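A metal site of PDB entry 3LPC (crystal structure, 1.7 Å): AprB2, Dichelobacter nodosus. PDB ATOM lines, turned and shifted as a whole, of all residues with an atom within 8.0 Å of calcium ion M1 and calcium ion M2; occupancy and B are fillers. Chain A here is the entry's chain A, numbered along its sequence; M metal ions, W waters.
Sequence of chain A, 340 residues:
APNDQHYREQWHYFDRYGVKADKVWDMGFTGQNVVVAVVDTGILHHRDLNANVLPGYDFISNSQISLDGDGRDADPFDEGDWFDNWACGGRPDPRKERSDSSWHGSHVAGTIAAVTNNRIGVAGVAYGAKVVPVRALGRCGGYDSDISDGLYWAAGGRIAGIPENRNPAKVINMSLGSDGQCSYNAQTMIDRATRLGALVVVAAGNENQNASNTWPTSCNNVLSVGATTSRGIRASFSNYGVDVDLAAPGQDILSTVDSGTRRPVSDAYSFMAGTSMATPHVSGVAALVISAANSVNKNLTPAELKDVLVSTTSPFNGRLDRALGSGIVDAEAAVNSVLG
The backbone carbonyl oxygen (O) of Asp 70 lies close to the side-chain hydroxyl (OG) of Ser 66. OD2 of Asp 58 sits close to NH1 of Arg 135. The backbone NH (N) of Asp 68 sits close to the side-chain hydroxyl (OG) of Ser 66, at 3.4 Å. The side-chain carboxylate (OD1) of Asp 58 lies within hydrogen-bond range of the backbone NH (N) of Ile 60. NH1 of Arg 135 lies close to OD2 of Asp 68 (3.8 Å). The side-chain carboxylate (OD1) of Asp 75 sits at hydrogen-bond distance from the backbone NH (N) of Phe 77, 3.0 Å away.
Four residues have an atom within 4 Å of calcium ion M1: Asp 68, Asp 70, Gly 71 and Asp 73.
Of the 23 residues printed, 4 come within 4 Å of calcium ion M2. The nearest printed residue that does not touch calcium ion M2 is Arg 135 (4.2 Å).
The backbone carbonyl oxygen (O) of Gly 71 binds calcium ion M1 (2.3 Å). OD1 of Asp 70 is bound to calcium ion M1 (2.3 Å). OD1 of Asp 73 is bound to calcium ion M1, 2.3 Å away. Water W3 is bound to calcium ion M1 (2.3 Å). OD1 of Asp 68 binds calcium ion M1 (2.5 Å). O of Asp 70 binds calcium ion M1, at 2.5 Å. OD2 of Asp 68 binds calcium ion M1 (2.5 Å).
Calcium ion M2 is bound by the side-chain carboxylate (OD2) of Asp 68 (2.3 Å), the backbone carbonyl oxygen (O) of Asp 75 (2.4 Å), water W1 (2.4 Å), the side-chain carboxylate (OD2) of Asp 58 (2.4 Å), water W2 (2.4 Å), the side-chain carboxylate (OD2) of Asp 73 (2.5 Å) and the side-chain carboxylate (OD1) of Asp 73 (2.6 Å).
Water W3 bridges the backbone carbonyl oxygen (O) of Ile 60 and the side-chain carboxylate (OD1) of Asp 58. Water W2 lies within hydrogen-bond range of OE2 of Glu 79, O of Phe 77 and NH1 of Arg 135.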
ATOM      1  N   TYR A  57      17.937  20.204  23.707  1.00  0.00           N
ATOM      2  CA  TYR A  57      18.796  21.332  23.340  1.00  0.00           C
ATOM      3  C   TYR A  57      18.437  21.793  21.943  1.00  0.00           C
ATOM      4  O   TYR A  57      17.963  20.995  21.140  1.00  0.00           O
ATOM      5  CB  TYR A  57      20.289  20.995  23.473  1.00  0.00           C
ATOM      6  CG  TYR A  57      21.115  22.222  23.810  1.00  0.00           C
ATOM      7  CD1 TYR A  57      21.311  22.598  25.135  1.00  0.00           C
ATOM      8  CD2 TYR A  57      21.678  23.012  22.810  1.00  0.00           C
ATOM      9  CE1 TYR A  57      22.052  23.749  25.455  1.00  0.00           C
ATOM     10  CE2 TYR A  57      22.419  24.172  23.126  1.00  0.00           C
ATOM     11  CZ  TYR A  57      22.596  24.524  24.450  1.00  0.00           C
ATOM     12  OH  TYR A  57      23.315  25.644  24.796  1.00  0.00           O
ATOM     13  N   ASP A  58      18.598  23.090  21.685  1.00  0.00           N
ATOM     14  CA  ASP A  58      18.231  23.672  20.381  1.00  0.00           C
ATOM     15  C   ASP A  58      19.519  23.927  19.601  1.00  0.00           C
ATOM     16  O   ASP A  58      20.317  24.787  19.979  1.00  0.00           O
ATOM     17  CB  ASP A  58      17.451  24.984  20.617  1.00  0.00           C
ATOM     18  CG  ASP A  58      16.797  25.521  19.364  1.00  0.00           C
ATOM     19  OD1 ASP A  58      17.286  25.265  18.239  1.00  0.00           O
ATOM     20  OD2 ASP A  58      15.793  26.249  19.515  1.00  0.00           O
ATOM     21  N   PHE A  59      19.732  23.143  18.547  1.00  0.00           N
ATOM     22  CA  PHE A  59      20.925  23.189  17.720  1.00  0.00           C
ATOM     23  C   PHE A  59      20.794  24.091  16.503  1.00  0.00           C
ATOM     24  O   PHE A  59      21.734  24.201  15.739  1.00  0.00           O
ATOM     25  CB  PHE A  59      21.312  21.774  17.283  1.00  0.00           C
ATOM     26  CG  PHE A  59      22.072  21.043  18.338  1.00  0.00           C
ATOM     27  CD1 PHE A  59      23.467  21.016  18.327  1.00  0.00           C
ATOM     28  CD2 PHE A  59      21.382  20.434  19.389  1.00  0.00           C
ATOM     29  CE1 PHE A  59      24.177  20.365  19.340  1.00  0.00           C
ATOM     30  CE2 PHE A  59      22.082  19.774  20.406  1.00  0.00           C
ATOM     31  CZ  PHE A  59      23.478  19.747  20.394  1.00  0.00           C
ATOM     32  N   ILE A  60      19.643  24.746  16.335  1.00  0.00           N
ATOM     33  CA  ILE A  60      19.477  25.617  15.165  1.00  0.00           C
ATOM     34  C   ILE A  60      20.358  26.862  15.292  1.00  0.00           C
ATOM     35  O   ILE A  60      20.212  27.650  16.214  1.00  0.00           O
ATOM     36  CB  ILE A  60      18.004  26.039  14.918  1.00  0.00           C
ATOM     37  CG1 ILE A  60      17.094  24.814  14.764  1.00  0.00           C
ATOM     38  CG2 ILE A  60      17.935  26.877  13.631  1.00  0.00           C
ATOM     39  CD1 ILE A  60      15.585  25.176  14.673  1.00  0.00           C
ATOM     40  N   SER A  61      21.279  27.038  14.337  1.00  0.00           N
ATOM     41  CA  SER A  61      22.259  28.104  14.394  1.00  0.00           C
ATOM     42  C   SER A  61      21.779  29.457  13.842  1.00  0.00           C
ATOM     43  O   SER A  61      22.281  30.504  14.253  1.00  0.00           O
ATOM     44  CB  SER A  61      23.517  27.672  13.639  1.00  0.00           C
ATOM     45  OG  SER A  61      24.143  26.617  14.359  1.00  0.00           O
ATOM     46  N   ASN A  62      20.842  29.416  12.896  1.00  0.00           N
ATOM     47  CA  ASN A  62      20.381  30.603  12.173  1.00  0.00           C
ATOM     48  C   ASN A  62      19.018  31.038  12.725  1.00  0.00           C
ATOM     49  O   ASN A  62      18.060  30.252  12.698  1.00  0.00           O
ATOM     50  CB  ASN A  62      20.305  30.269  10.681  1.00  0.00           C
ATOM     51  CG  ASN A  62      19.934  31.444   9.817  1.00  0.00           C
ATOM     52  OD1 ASN A  62      19.333  32.416  10.274  1.00  0.00           O
ATOM     53  ND2 ASN A  62      20.302  31.367   8.537  1.00  0.00           N
ATOM     54  N   SER A  63      18.950  32.261  13.262  1.00  0.00           N
ATOM     55  CA  SER A  63      17.717  32.771  13.871  1.00  0.00           C
ATOM     56  C   SER A  63      16.565  32.924  12.875  1.00  0.00           C
ATOM     57  O   SER A  63      15.390  32.964  13.285  1.00  0.00           O
ATOM     58  CB  SER A  63      17.973  34.085  14.604  1.00  0.00           C
ATOM     59  OG  SER A  63      18.464  35.070  13.703  1.00  0.00           O
ATOM     60  N   ILE A  65      15.816  30.653  10.834  1.00  0.00           N
ATOM     61  CA  ILE A  65      15.216  29.318  10.825  1.00  0.00           C
ATOM     62  C   ILE A  65      14.574  28.997  12.184  1.00  0.00           C
ATOM     63  O   ILE A  65      13.474  28.434  12.240  1.00  0.00           O
ATOM     64  CB  ILE A  65      16.266  28.222  10.450  1.00  0.00           C
ATOM     65  CG1 ILE A  65      16.799  28.463   9.027  1.00  0.00           C
ATOM     66  CG2 ILE A  65      15.667  26.807  10.626  1.00  0.00           C
ATOM     67  CD1 ILE A  65      18.002  27.582   8.634  1.00  0.00           C
ATOM     68  N   SER A  66      15.256  29.362  13.266  1.00  0.00           N
ATOM     69  CA  SER A  66      14.840  29.005  14.611  1.00  0.00           C
ATOM     70  C   SER A  66      13.594  29.753  15.072  1.00  0.00           C
ATOM     71  O   SER A  66      12.811  29.234  15.872  1.00  0.00           O
ATOM     72  CB  SER A  66      15.970  29.299  15.606  1.00  0.00           C
ATOM     73  OG  SER A  66      16.178  30.700  15.736  1.00  0.00           O
ATOM     74  N   LEU A  67      13.445  30.984  14.582  1.00  0.00           N
ATOM     75  CA  LEU A  67      12.344  31.878  14.960  1.00  0.00           C
ATOM     76  C   LEU A  67      12.268  32.140  16.482  1.00  0.00           C
ATOM     77  O   LEU A  67      11.206  32.452  17.011  1.00  0.00           O
ATOM     78  CB  LEU A  67      11.004  31.353  14.424  1.00  0.00           C
ATOM     79  CG  LEU A  67      10.916  31.168  12.891  1.00  0.00           C
ATOM     80  CD1 LEU A  67       9.482  30.741  12.504  1.00  0.00           C
ATOM     81  CD2 LEU A  67      11.323  32.396  12.152  1.00  0.00           C
ATOM     82  N   ASP A  68      13.407  32.042  17.167  1.00  0.00           N
ATOM     83  CA  ASP A  68      13.413  32.290  18.605  1.00  0.00           C
ATOM     84  C   ASP A  68      14.422  33.397  18.980  1.00  0.00           C
ATOM     85  O   ASP A  68      14.747  33.573  20.161  1.00  0.00           O
ATOM     86  CB  ASP A  68      13.693  30.980  19.369  1.00  0.00           C
ATOM     87  CG  ASP A  68      15.110  30.445  19.150  1.00  0.00           C
ATOM     88  OD1 ASP A  68      15.929  31.116  18.479  1.00  0.00           O
ATOM     89  OD2 ASP A  68      15.393  29.341  19.647  1.00  0.00           O
ATOM     90  N   GLY A  69      14.937  34.100  17.988  1.00  0.00           N
ATOM     91  CA  GLY A  69      15.757  35.295  18.226  1.00  0.00           C
ATOM     92  C   GLY A  69      17.245  35.091  18.352  1.00  0.00           C
ATOM     93  O   GLY A  69      17.996  36.063  18.416  1.00  0.00           O
ATOM     94  N   ASP A  70      17.703  33.836  18.405  1.00  0.00           N
ATOM     95  CA  ASP A  70      19.121  33.571  18.625  1.00  0.00           C
ATOM     96  C   ASP A  70      19.534  32.221  18.039  1.00  0.00           C
ATOM     97  O   ASP A  70      18.682  31.460  17.573  1.00  0.00           O
ATOM     98  CB  ASP A  70      19.499  33.677  20.131  1.00  0.00           C
ATOM     99  CG  ASP A  70      18.799  32.661  21.029  1.00  0.00           C
ATOM    100  OD1 ASP A  70      18.159  31.707  20.554  1.00  0.00           O
ATOM    101  OD2 ASP A  70      18.895  32.822  22.275  1.00  0.00           O
ATOM    102  N   GLY A  71      20.825  31.936  18.076  1.00  0.00           N
ATOM    103  CA  GLY A  71      21.358  30.653  17.634  1.00  0.00           C
ATOM    104  C   GLY A  71      21.151  29.556  18.654  1.00  0.00           C
ATOM    105  O   GLY A  71      20.102  29.472  19.317  1.00  0.00           O
ATOM    106  N   ARG A  72      22.146  28.695  18.776  1.00  0.00           N
ATOM    107  CA  ARG A  72      21.972  27.524  19.645  1.00  0.00           C
ATOM    108  C   ARG A  72      21.650  27.950  21.059  1.00  0.00           C
ATOM    109  O   ARG A  72      22.215  28.920  21.559  1.00  0.00           O
ATOM    110  CB  ARG A  72      23.205  26.631  19.578  1.00  0.00           C
ATOM    111  CG  ARG A  72      23.432  26.119  18.151  1.00  0.00           C
ATOM    112  CD  ARG A  72      24.487  25.029  18.133  1.00  0.00           C
ATOM    113  NE  ARG A  72      24.565  24.387  16.816  1.00  0.00           N
ATOM    114  CZ  ARG A  72      25.521  23.538  16.448  1.00  0.00           C
ATOM    115  NH1 ARG A  72      26.518  23.253  17.287  1.00  0.00           N
ATOM    116  NH2 ARG A  72      25.501  23.000  15.230  1.00  0.00           N
ATOM    117  N   ASP A  73      20.716  27.237  21.690  1.00  0.00           N
ATOM    118  CA  ASP A  73      20.234  27.634  23.026  1.00  0.00           C
ATOM    119  C   ASP A  73      19.646  26.442  23.739  1.00  0.00           C
ATOM    120  O   ASP A  73      19.350  25.423  23.123  1.00  0.00           O
ATOM    121  CB  ASP A  73      19.210  28.787  22.932  1.00  0.00           C
ATOM    122  CG  ASP A  73      17.873  28.341  22.351  1.00  0.00           C
ATOM    123  OD1 ASP A  73      17.693  28.436  21.109  1.00  0.00           O
ATOM    124  OD2 ASP A  73      16.993  27.864  23.100  1.00  0.00           O
ATOM    125  N   ALA A  74      19.431  26.580  25.054  1.00  0.00           N
ATOM    126  CA  ALA A  74      19.009  25.446  25.876  1.00  0.00           C
ATOM    127  C   ALA A  74      17.546  25.047  25.783  1.00  0.00           C
ATOM    128  O   ALA A  74      17.135  24.080  26.454  1.00  0.00           O
ATOM    129  CB  ALA A  74      19.418  25.680  27.327  1.00  0.00           C
ATOM    130  N   ASP A  75      16.755  25.773  24.981  1.00  0.00           N
ATOM    131  CA  ASP A  75      15.308  25.553  24.939  1.00  0.00           C
ATOM    132  C   ASP A  75      14.850  25.048  23.577  1.00  0.00           C
ATOM    133  O   ASP A  75      14.782  25.832  22.623  1.00  0.00           O
ATOM    134  CB  ASP A  75      14.556  26.848  25.271  1.00  0.00           C
ATOM    135  CG  ASP A  75      13.045  26.649  25.324  1.00  0.00           C
ATOM    136  OD1 ASP A  75      12.572  25.502  25.124  1.00  0.00           O
ATOM    137  OD2 ASP A  75      12.320  27.649  25.560  1.00  0.00           O
ATOM    138  N   PRO A  76      14.544  23.734  23.475  1.00  0.00           N
ATOM    139  CA  PRO A  76      14.214  23.152  22.165  1.00  0.00           C
ATOM    140  C   PRO A  76      12.717  23.264  21.834  1.00  0.00           C
ATOM    141  O   PRO A  76      12.187  22.456  21.073  1.00  0.00           O
ATOM    142  CB  PRO A  76      14.614  21.682  22.365  1.00  0.00           C
ATOM    143  CG  PRO A  76      14.215  21.410  23.780  1.00  0.00           C
ATOM    144  CD  PRO A  76      14.623  22.691  24.520  1.00  0.00           C
ATOM    145  N   PHE A  77      12.049  24.271  22.412  1.00  0.00           N
ATOM    146  CA  PHE A  77      10.656  24.526  22.074  1.00  0.00           C
ATOM    147  C   PHE A  77      10.480  24.669  20.550  1.00  0.00           C
ATOM    148  O   PHE A  77      11.260  25.338  19.874  1.00  0.00           O
ATOM    149  CB  PHE A  77      10.139  25.776  22.804  1.00  0.00           C
ATOM    150  CG  PHE A  77       8.663  25.976  22.670  1.00  0.00           C
ATOM    151  CD1 PHE A  77       7.773  25.127  23.327  1.00  0.00           C
ATOM    152  CD2 PHE A  77       8.149  27.005  21.867  1.00  0.00           C
ATOM    153  CE1 PHE A  77       6.400  25.294  23.182  1.00  0.00           C
ATOM    154  CE2 PHE A  77       6.776  27.177  21.730  1.00  0.00           C
ATOM    155  CZ  PHE A  77       5.907  26.315  22.386  1.00  0.00           C
ATOM    156  N   ASP A  78       9.439  24.036  20.016  1.00  0.00           N
ATOM    157  CA  ASP A  78       9.129  24.170  18.593  1.00  0.00           C
ATOM    158  C   ASP A  78       8.335  25.479  18.458  1.00  0.00           C
ATOM    159  O   ASP A  78       7.160  25.533  18.790  1.00  0.00           O
ATOM    160  CB  ASP A  78       8.296  22.964  18.150  1.00  0.00           C
ATOM    161  CG  ASP A  78       7.982  22.964  16.651  1.00  0.00           C
ATOM    162  OD1 ASP A  78       8.217  24.001  15.995  1.00  0.00           O
ATOM    163  OD2 ASP A  78       7.502  21.939  16.138  1.00  0.00           O
ATOM    164  N   GLU A  79       8.997  26.514  17.938  1.00  0.00           N
ATOM    165  CA  GLU A  79       8.366  27.825  17.792  1.00  0.00           C
ATOM    166  C   GLU A  79       7.259  27.789  16.748  1.00  0.00           C
ATOM    167  O   GLU A  79       6.422  28.706  16.712  1.00  0.00           O
ATOM    168  CB  GLU A  79       9.398  28.872  17.370  1.00  0.00           C
ATOM    169  CG  GLU A  79      10.608  28.972  18.289  1.00  0.00           C
ATOM    170  CD  GLU A  79      10.296  29.456  19.684  1.00  0.00           C
ATOM    171  OE1 GLU A  79       9.309  30.217  19.853  1.00  0.00           O
ATOM    172  OE2 GLU A  79      11.061  29.109  20.626  1.00  0.00           O
ATOM    173  N   ARG A 135      16.366  19.896  18.882  1.00  0.00           N
ATOM    174  CA  ARG A 135      15.778  20.757  17.861  1.00  0.00           C
ATOM    175  C   ARG A 135      16.838  21.145  16.842  1.00  0.00           C
ATOM    176  O   ARG A 135      17.802  21.844  17.163  1.00  0.00           O
ATOM    177  CB  ARG A 135      15.145  21.992  18.477  1.00  0.00           C
ATOM    178  CG  ARG A 135      14.476  22.911  17.433  1.00  0.00           C
ATOM    179  CD  ARG A 135      13.624  23.987  18.083  1.00  0.00           C
ATOM    180  NE  ARG A 135      12.775  24.674  17.109  1.00  0.00           N
ATOM    181  CZ  ARG A 135      12.800  26.003  16.881  1.00  0.00           C
ATOM    182  NH1 ARG A 135      13.661  26.794  17.505  1.00  0.00           N
ATOM    183  NH2 ARG A 135      11.946  26.543  16.012  1.00  0.00           N
HETATM  184 CA    CA M   1      17.860  29.827  19.266  1.00  0.00          CA
HETATM  185 CA    CA M   2      15.244  27.706  21.282  1.00  0.00          CA
HETATM  186  O   HOH W   1      14.353  29.409  22.637  1.00  0.00           O
HETATM  187  O   HOH W   2      12.947  27.348  20.677  1.00  0.00           O
HETATM  188  O   HOH W   3      18.015  28.046  17.783  1.00  0.00           O
